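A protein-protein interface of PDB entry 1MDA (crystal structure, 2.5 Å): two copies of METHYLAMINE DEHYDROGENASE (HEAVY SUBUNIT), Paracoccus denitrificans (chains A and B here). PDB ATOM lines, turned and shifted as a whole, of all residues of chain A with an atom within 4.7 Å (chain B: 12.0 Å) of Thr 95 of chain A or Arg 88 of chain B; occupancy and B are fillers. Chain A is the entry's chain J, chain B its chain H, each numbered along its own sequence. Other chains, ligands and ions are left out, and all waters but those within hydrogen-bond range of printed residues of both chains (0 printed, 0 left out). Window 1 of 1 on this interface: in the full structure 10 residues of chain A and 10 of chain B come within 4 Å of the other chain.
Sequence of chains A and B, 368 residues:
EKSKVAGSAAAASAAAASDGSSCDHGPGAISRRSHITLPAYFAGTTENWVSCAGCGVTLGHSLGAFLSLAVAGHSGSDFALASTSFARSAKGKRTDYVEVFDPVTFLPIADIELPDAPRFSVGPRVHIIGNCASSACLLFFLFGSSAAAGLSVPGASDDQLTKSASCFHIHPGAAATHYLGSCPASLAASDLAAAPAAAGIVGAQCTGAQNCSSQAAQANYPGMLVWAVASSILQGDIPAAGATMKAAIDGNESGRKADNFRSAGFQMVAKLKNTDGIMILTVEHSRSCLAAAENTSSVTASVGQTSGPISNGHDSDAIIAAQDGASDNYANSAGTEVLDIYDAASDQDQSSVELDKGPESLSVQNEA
The side-chain carboxylate (OD2) of Asp 111 of chain A is in salt-bridge range of the guanidinium group (NH1) of Arg 88 of chain B, at 2.4 Å.
The backbone NH (N) of Tyr 97 of chain A is in hydrogen-bond range of the backbone carbonyl oxygen (O) of Ser 83 of chain A (2.7 Å).
The backbone carbonyl oxygen of Ser 85 of chain A lies within hydrogen-bond range of the backbone NH of Thr 95 of chain A, at 2.7 Å.
CG2 of Thr 95 of chain A touches NH2 of Arg 88 of chain B (3.8 Å).
CG of Tyr 97 of chain A touches NH1 of Arg 88 of chain B, at 3.97 Å.
Thr 95 of chain A touches just one residue of chain B: Arg 88 (3.8 Å).
Arg 88 of chain B touches just these residues of chain A: Thr 95 (3.8 Å), Tyr 97 (3.97 Å) and Asp 111 (2.4 Å).
No residue of chain B comes within 4 Å of Ser 83 of chain A.
No residue of chain B comes within 4 Å of Thr 84 of chain A.
No residue of chain B comes within 4 Å of Ser 85 of chain A.
No residue of chain B comes within 4 Å of Lys 93 of chain A.
Arg 94 of chain A touches none of the printed residues of chain B.
No residue of chain B comes within 4 Å of Asp 96 of chain A.
No residue of chain B comes within 4 Å of Glu 113 of chain A.
Ala 65 of chain B touches none of the printed residues of chain A.
The nearest residue of chain B that does not touch Thr 95 of chain A is Ala 87 of chain B (8.0 Å).
Hydrophobic or aromatic side chains of chain A within 4 Å of the printed part of chain B: Tyr 97.
Among the printed residues, 3 pairs touch across the chains.
Positions printed for both chains: 84, 85, 93, 94, 95 and 97.
Of the 3 pairs that touch across the chains among the printed residues, none has its exchanged pair printed and touching as well.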
ATOM      1  N   SER A  83      19.908   2.418  -0.403  1.00  0.00           N
ATOM      2  CA  SER A  83      19.027   3.182   0.459  1.00  0.00           C
ATOM      3  C   SER A  83      17.552   2.791   0.443  1.00  0.00           C
ATOM      4  O   SER A  83      17.098   2.067  -0.436  1.00  0.00           O
ATOM      5  CB  SER A  83      19.286   4.680   0.190  1.00  0.00           C
ATOM      6  OG  SER A  83      18.355   5.565   0.807  1.00  0.00           O
ATOM      7  N   THR A  84      16.829   3.328   1.434  1.00  0.00           N
ATOM      8  CA  THR A  84      15.434   3.068   1.688  1.00  0.00           C
ATOM      9  C   THR A  84      14.649   4.300   2.061  1.00  0.00           C
ATOM     10  O   THR A  84      14.928   4.968   3.052  1.00  0.00           O
ATOM     11  CB  THR A  84      15.327   2.102   2.876  1.00  0.00           C
ATOM     12  OG1 THR A  84      15.756   0.837   2.464  1.00  0.00           O
ATOM     13  CG2 THR A  84      13.926   2.059   3.464  1.00  0.00           C
ATOM     14  N   SER A  85      13.524   4.427   1.380  1.00  0.00           N
ATOM     15  CA  SER A  85      12.581   5.495   1.582  1.00  0.00           C
ATOM     16  C   SER A  85      11.205   4.872   1.645  1.00  0.00           C
ATOM     17  O   SER A  85      11.007   3.742   1.216  1.00  0.00           O
ATOM     18  CB  SER A  85      12.652   6.531   0.456  1.00  0.00           C
ATOM     19  OG  SER A  85      13.841   7.292   0.572  1.00  0.00           O
ATOM     20  N   LYS A  93       4.511   2.878   1.523  1.00  0.00           N
ATOM     21  CA  LYS A  93       5.312   2.042   0.662  1.00  0.00           C
ATOM     22  C   LYS A  93       6.783   2.309   0.834  1.00  0.00           C
ATOM     23  O   LYS A  93       7.258   3.436   0.841  1.00  0.00           O
ATOM     24  CB  LYS A  93       4.907   2.167  -0.790  1.00  0.00           C
ATOM     25  CG  LYS A  93       5.161   0.898  -1.616  1.00  0.00           C
ATOM     26  CD  LYS A  93       6.526   0.760  -2.288  1.00  0.00           C
ATOM     27  CE  LYS A  93       6.664   1.626  -3.545  1.00  0.00           C
ATOM     28  NZ  LYS A  93       5.592   1.390  -4.533  1.00  0.00           N
ATOM     29  N   ARG A  94       7.475   1.216   0.982  1.00  0.00           N
ATOM     30  CA  ARG A  94       8.901   1.209   1.125  1.00  0.00           C
ATOM     31  C   ARG A  94       9.553   0.993  -0.209  1.00  0.00           C
ATOM     32  O   ARG A  94       9.083   0.195  -1.010  1.00  0.00           O
ATOM     33  CB  ARG A  94       9.349   0.132   2.115  1.00  0.00           C
ATOM     34  CG  ARG A  94      10.800  -0.194   1.955  1.00  0.00           C
ATOM     35  CD  ARG A  94      11.280  -1.143   3.021  1.00  0.00           C
ATOM     36  NE  ARG A  94      12.706  -1.436   2.987  1.00  0.00           N
ATOM     37  CZ  ARG A  94      13.226  -2.395   3.746  1.00  0.00           C
ATOM     38  NH1 ARG A  94      12.458  -3.121   4.545  1.00  0.00           N
ATOM     39  NH2 ARG A  94      14.528  -2.635   3.703  1.00  0.00           N
ATOM     40  N   THR A  95      10.689   1.628  -0.400  1.00  0.00           N
ATOM     41  CA  THR A  95      11.423   1.491  -1.619  1.00  0.00           C
ATOM     42  C   THR A  95      12.883   1.454  -1.277  1.00  0.00           C
ATOM     43  O   THR A  95      13.352   2.349  -0.589  1.00  0.00           O
ATOM     44  CB  THR A  95      11.269   2.709  -2.552  1.00  0.00           C
ATOM     45  OG1 THR A  95       9.897   2.972  -2.756  1.00  0.00           O
ATOM     46  CG2 THR A  95      11.973   2.457  -3.912  1.00  0.00           C
ATOM     47  N   ASP A  96      13.554   0.380  -1.701  1.00  0.00           N
ATOM     48  CA  ASP A  96      14.987   0.253  -1.540  1.00  0.00           C
ATOM     49  C   ASP A  96      15.588   0.578  -2.881  1.00  0.00           C
ATOM     50  O   ASP A  96      14.960   0.271  -3.887  1.00  0.00           O
ATOM     51  CB  ASP A  96      15.459  -1.127  -1.078  1.00  0.00           C
ATOM     52  CG  ASP A  96      14.994  -1.539   0.292  1.00  0.00           C
ATOM     53  OD1 ASP A  96      14.599  -0.539   1.051  1.00  0.00           O
ATOM     54  OD2 ASP A  96      14.979  -2.697   0.633  1.00  0.00           O
ATOM     55  N   TYR A  97      16.784   1.150  -2.917  1.00  0.00           N
ATOM     56  CA  TYR A  97      17.388   1.521  -4.194  1.00  0.00           C
ATOM     57  C   TYR A  97      18.882   1.746  -4.062  1.00  0.00           C
ATOM     58  O   TYR A  97      19.424   1.945  -2.985  1.00  0.00           O
ATOM     59  CB  TYR A  97      16.725   2.790  -4.783  1.00  0.00           C
ATOM     60  CG  TYR A  97      16.806   3.980  -3.844  1.00  0.00           C
ATOM     61  CD1 TYR A  97      15.863   4.153  -2.832  1.00  0.00           C
ATOM     62  CD2 TYR A  97      17.853   4.908  -3.934  1.00  0.00           C
ATOM     63  CE1 TYR A  97      15.950   5.226  -1.939  1.00  0.00           C
ATOM     64  CE2 TYR A  97      17.973   5.974  -3.039  1.00  0.00           C
ATOM     65  CZ  TYR A  97      17.009   6.131  -2.038  1.00  0.00           C
ATOM     66  OH  TYR A  97      17.104   7.195  -1.160  1.00  0.00           O
ATOM     67  N   ASP A 111      20.006   5.570 -10.548  1.00  0.00           N
ATOM     68  CA  ASP A 111      19.076   5.269  -9.464  1.00  0.00           C
ATOM     69  C   ASP A 111      18.470   3.933  -9.839  1.00  0.00           C
ATOM     70  O   ASP A 111      17.769   3.835 -10.855  1.00  0.00           O
ATOM     71  CB  ASP A 111      17.984   6.357  -9.250  1.00  0.00           C
ATOM     72  CG  ASP A 111      17.018   6.123  -8.090  1.00  0.00           C
ATOM     73  OD1 ASP A 111      16.394   4.964  -8.129  1.00  0.00           O
ATOM     74  OD2 ASP A 111      16.762   6.964  -7.241  1.00  0.00           O
ATOM     75  N   GLU A 113      16.433   0.485  -8.512  1.00  0.00           N
ATOM     76  CA  GLU A 113      15.565  -0.044  -7.480  1.00  0.00           C
ATOM     77  C   GLU A 113      15.788  -1.502  -7.149  1.00  0.00           C
ATOM     78  O   GLU A 113      16.052  -2.333  -8.011  1.00  0.00           O
ATOM     79  CB  GLU A 113      14.067   0.205  -7.754  1.00  0.00           C
ATOM     80  CG  GLU A 113      13.730   1.692  -7.922  1.00  0.00           C
ATOM     81  CD  GLU A 113      12.253   1.981  -7.892  1.00  0.00           C
ATOM     82  OE1 GLU A 113      11.518   0.877  -7.883  1.00  0.00           O
ATOM     83  OE2 GLU A 113      11.794   3.122  -7.860  1.00  0.00           O
ATOM     84  N   ALA B  43      14.123  21.293   8.079  1.00  0.00           N
ATOM     85  CA  ALA B  43      14.476  19.964   7.636  1.00  0.00           C
ATOM     86  C   ALA B  43      13.330  19.333   6.856  1.00  0.00           C
ATOM     87  O   ALA B  43      12.150  19.568   7.140  1.00  0.00           O
ATOM     88  CB  ALA B  43      14.949  19.076   8.751  1.00  0.00           C
ATOM     89  N   GLY B  44      13.709  18.502   5.900  1.00  0.00           N
ATOM     90  CA  GLY B  44      12.788  17.790   5.044  1.00  0.00           C
ATOM     91  C   GLY B  44      11.742  16.975   5.813  1.00  0.00           C
ATOM     92  O   GLY B  44      10.632  16.748   5.337  1.00  0.00           O
ATOM     93  N   THR B  45      12.053  16.610   7.037  1.00  0.00           N
ATOM     94  CA  THR B  45      11.163  15.817   7.844  1.00  0.00           C
ATOM     95  C   THR B  45      11.000  16.493   9.183  1.00  0.00           C
ATOM     96  O   THR B  45      11.971  17.046   9.712  1.00  0.00           O
ATOM     97  CB  THR B  45      11.725  14.388   8.063  1.00  0.00           C
ATOM     98  OG1 THR B  45      11.650  13.636   6.859  1.00  0.00           O
ATOM     99  CG2 THR B  45      11.015  13.694   9.233  1.00  0.00           C
ATOM    100  N   ALA B  65       6.225  16.169   7.176  1.00  0.00           N
ATOM    101  CA  ALA B  65       7.330  16.522   6.314  1.00  0.00           C
ATOM    102  C   ALA B  65       7.799  17.958   6.316  1.00  0.00           C
ATOM    103  O   ALA B  65       8.074  18.539   7.365  1.00  0.00           O
ATOM    104  CB  ALA B  65       7.360  15.831   4.974  1.00  0.00           C
ATOM    105  N   PHE B  66       7.995  18.464   5.101  1.00  0.00           N
ATOM    106  CA  PHE B  66       8.556  19.792   4.913  1.00  0.00           C
ATOM    107  C   PHE B  66       7.581  20.914   5.180  1.00  0.00           C
ATOM    108  O   PHE B  66       6.574  21.105   4.501  1.00  0.00           O
ATOM    109  CB  PHE B  66       9.376  19.898   3.591  1.00  0.00           C
ATOM    110  CG  PHE B  66      10.060  21.207   3.257  1.00  0.00           C
ATOM    111  CD1 PHE B  66      11.039  21.739   4.098  1.00  0.00           C
ATOM    112  CD2 PHE B  66       9.766  21.901   2.082  1.00  0.00           C
ATOM    113  CE1 PHE B  66      11.693  22.933   3.785  1.00  0.00           C
ATOM    114  CE2 PHE B  66      10.406  23.095   1.753  1.00  0.00           C
ATOM    115  CZ  PHE B  66      11.366  23.618   2.619  1.00  0.00           C
ATOM    116  N   THR B  84       4.162  18.013   2.797  1.00  0.00           N
ATOM    117  CA  THR B  84       4.916  17.905   1.572  1.00  0.00           C
ATOM    118  C   THR B  84       6.021  16.883   1.686  1.00  0.00           C
ATOM    119  O   THR B  84       6.939  17.030   2.499  1.00  0.00           O
ATOM    120  CB  THR B  84       5.539  19.251   1.170  1.00  0.00           C
ATOM    121  OG1 THR B  84       4.560  20.269   1.143  1.00  0.00           O
ATOM    122  CG2 THR B  84       6.177  19.102  -0.189  1.00  0.00           C
ATOM    123  N   SER B  85       6.020  16.000   0.691  1.00  0.00           N
ATOM    124  CA  SER B  85       6.964  14.907   0.547  1.00  0.00           C
ATOM    125  C   SER B  85       7.639  14.908  -0.835  1.00  0.00           C
ATOM    126  O   SER B  85       7.114  15.450  -1.806  1.00  0.00           O
ATOM    127  CB  SER B  85       6.214  13.597   0.738  1.00  0.00           C
ATOM    128  OG  SER B  85       5.846  13.440   2.097  1.00  0.00           O
ATOM    129  N   PHE B  86       8.819  14.287  -0.946  1.00  0.00           N
ATOM    130  CA  PHE B  86       9.500  14.200  -2.239  1.00  0.00           C
ATOM    131  C   PHE B  86      10.003  12.780  -2.409  1.00  0.00           C
ATOM    132  O   PHE B  86      10.279  12.075  -1.439  1.00  0.00           O
ATOM    133  CB  PHE B  86      10.710  15.134  -2.390  1.00  0.00           C
ATOM    134  CG  PHE B  86      10.434  16.541  -1.993  1.00  0.00           C
ATOM    135  CD1 PHE B  86      10.531  16.914  -0.653  1.00  0.00           C
ATOM    136  CD2 PHE B  86      10.065  17.500  -2.939  1.00  0.00           C
ATOM    137  CE1 PHE B  86      10.261  18.221  -0.249  1.00  0.00           C
ATOM    138  CE2 PHE B  86       9.775  18.815  -2.552  1.00  0.00           C
ATOM    139  CZ  PHE B  86       9.879  19.165  -1.202  1.00  0.00           C
ATOM    140  N   ALA B  87      10.032  12.304  -3.640  1.00  0.00           N
ATOM    141  CA  ALA B  87      10.551  10.973  -3.833  1.00  0.00           C
ATOM    142  C   ALA B  87      12.051  11.140  -3.727  1.00  0.00           C
ATOM    143  O   ALA B  87      12.583  11.857  -4.551  1.00  0.00           O
ATOM    144  CB  ALA B  87      10.157  10.550  -5.232  1.00  0.00           C
ATOM    145  N   ARG B  88      12.746  10.453  -2.832  1.00  0.00           N
ATOM    146  CA  ARG B  88      14.193  10.662  -2.633  1.00  0.00           C
ATOM    147  C   ARG B  88      14.338  11.942  -1.776  1.00  0.00           C
ATOM    148  O   ARG B  88      15.225  12.795  -2.000  1.00  0.00           O
ATOM    149  CB  ARG B  88      15.035  10.873  -3.907  1.00  0.00           C
ATOM    150  CG  ARG B  88      14.965   9.932  -5.117  1.00  0.00           C
ATOM    151  CD  ARG B  88      15.401   8.501  -4.839  1.00  0.00           C
ATOM    152  NE  ARG B  88      14.237   7.713  -4.522  1.00  0.00           N
ATOM    153  CZ  ARG B  88      13.832   6.714  -5.266  1.00  0.00           C
ATOM    154  NH1 ARG B  88      14.640   6.292  -6.229  1.00  0.00           N
ATOM    155  NH2 ARG B  88      12.713   6.040  -4.982  1.00  0.00           N
ATOM    156  N   SER B  89      13.472  12.016  -0.761  1.00  0.00           N
ATOM    157  CA  SER B  89      13.207  13.156   0.118  1.00  0.00           C
ATOM    158  C   SER B  89      14.224  14.229   0.307  1.00  0.00           C
ATOM    159  O   SER B  89      15.224  14.096   1.025  1.00  0.00           O
ATOM    160  CB  SER B  89      12.187  12.974   1.239  1.00  0.00           C
ATOM    161  OG  SER B  89      11.900  14.230   1.810  1.00  0.00           O
ATOM    162  N   ALA B  90      13.865  15.282  -0.397  1.00  0.00           N
ATOM    163  CA  ALA B  90      14.541  16.557  -0.568  1.00  0.00           C
ATOM    164  C   ALA B  90      14.554  16.794  -2.058  1.00  0.00           C
ATOM    165  O   ALA B  90      14.598  17.896  -2.542  1.00  0.00           O
ATOM    166  CB  ALA B  90      15.935  16.649   0.003  1.00  0.00           C
ATOM    167  N   LYS B  91      14.412  15.712  -2.806  1.00  0.00           N
ATOM    168  CA  LYS B  91      14.405  15.820  -4.251  1.00  0.00           C
ATOM    169  C   LYS B  91      13.465  14.810  -4.842  1.00  0.00           C
ATOM    170  O   LYS B  91      12.968  13.979  -4.099  1.00  0.00           O
ATOM    171  CB  LYS B  91      15.784  15.709  -4.891  1.00  0.00           C
ATOM    172  CG  LYS B  91      16.498  14.378  -4.654  1.00  0.00           C
ATOM    173  CD  LYS B  91      17.946  14.480  -5.115  1.00  0.00           C
ATOM    174  CE  LYS B  91      18.927  13.453  -4.553  1.00  0.00           C
ATOM    175  NZ  LYS B  91      19.088  12.232  -5.358  1.00  0.00           N
ATOM    176  N   GLY B  92      13.284  14.893  -6.166  1.00  0.00           N
ATOM    177  CA  GLY B  92      12.382  14.031  -6.920  1.00  0.00           C
ATOM    178  C   GLY B  92      10.981  14.639  -7.050  1.00  0.00           C
ATOM    179  O   GLY B  92      10.819  15.857  -6.971  1.00  0.00           O
ATOM    180  N   LYS B  93       9.989  13.788  -7.320  1.00  0.00           N
ATOM    181  CA  LYS B  93       8.584  14.162  -7.465  1.00  0.00           C
ATOM    182  C   LYS B  93       7.996  14.589  -6.121  1.00  0.00           C
ATOM    183  O   LYS B  93       8.054  13.837  -5.146  1.00  0.00           O
ATOM    184  CB  LYS B  93       7.798  12.986  -8.055  1.00  0.00           C
ATOM    185  CG  LYS B  93       6.536  13.350  -8.842  1.00  0.00           C
ATOM    186  CD  LYS B  93       5.253  13.532  -8.027  1.00  0.00           C
ATOM    187  CE  LYS B  93       4.346  12.289  -7.905  1.00  0.00           C
ATOM    188  NZ  LYS B  93       3.502  12.060  -9.101  1.00  0.00           N
ATOM    189  N   ARG B  94       7.469  15.821  -6.102  1.00  0.00           N
ATOM    190  CA  ARG B  94       6.852  16.439  -4.946  1.00  0.00           C
ATOM    191  C   ARG B  94       5.412  16.018  -4.806  1.00  0.00           C
ATOM    192  O   ARG B  94       4.700  15.914  -5.802  1.00  0.00           O
ATOM    193  CB  ARG B  94       6.954  17.958  -5.070  1.00  0.00           C
ATOM    194  CG  ARG B  94       6.204  18.738  -3.987  1.00  0.00           C
ATOM    195  CD  ARG B  94       6.300  20.242  -4.205  1.00  0.00           C
ATOM    196  NE  ARG B  94       5.432  21.028  -3.343  1.00  0.00           N
ATOM    197  CZ  ARG B  94       5.476  22.343  -3.342  1.00  0.00           C
ATOM    198  NH1 ARG B  94       6.323  22.998  -4.135  1.00  0.00           N
ATOM    199  NH2 ARG B  94       4.662  23.003  -2.544  1.00  0.00           N
ATOM    200  N   THR B  95       4.963  15.858  -3.570  1.00  0.00           N
ATOM    201  CA  THR B  95       3.567  15.544  -3.327  1.00  0.00           C
ATOM    202  C   THR B  95       3.071  16.323  -2.152  1.00  0.00           C
ATOM    203  O   THR B  95       3.656  16.202  -1.080  1.00  0.00           O
ATOM    204  CB  THR B  95       3.265  14.095  -2.967  1.00  0.00           C
ATOM    205  OG1 THR B  95       3.659  13.240  -3.998  1.00  0.00           O
ATOM    206  CG2 THR B  95       1.774  13.987  -2.702  1.00  0.00           C
ATOM    207  N   TYR B  97      -0.123  16.929   0.291  1.00  0.00           N
ATOM    208  CA  TYR B  97      -1.265  16.138   0.758  1.00  0.00           C
ATOM    209  C   TYR B  97      -1.732  16.600   2.126  1.00  0.00           C
ATOM    210  O   TYR B  97      -0.979  17.233   2.855  1.00  0.00           O
ATOM    211  CB  TYR B  97      -0.875  14.649   0.897  1.00  0.00           C
ATOM    212  CG  TYR B  97       0.286  14.467   1.853  1.00  0.00           C
ATOM    213  CD1 TYR B  97       1.590  14.668   1.386  1.00  0.00           C
ATOM    214  CD2 TYR B  97       0.112  14.127   3.199  1.00  0.00           C
ATOM    215  CE1 TYR B  97       2.700  14.517   2.221  1.00  0.00           C
ATOM    216  CE2 TYR B  97       1.209  13.988   4.053  1.00  0.00           C
ATOM    217  CZ  TYR B  97       2.504  14.187   3.567  1.00  0.00           C
ATOM    218  OH  TYR B  97       3.595  14.068   4.407  1.00  0.00           O
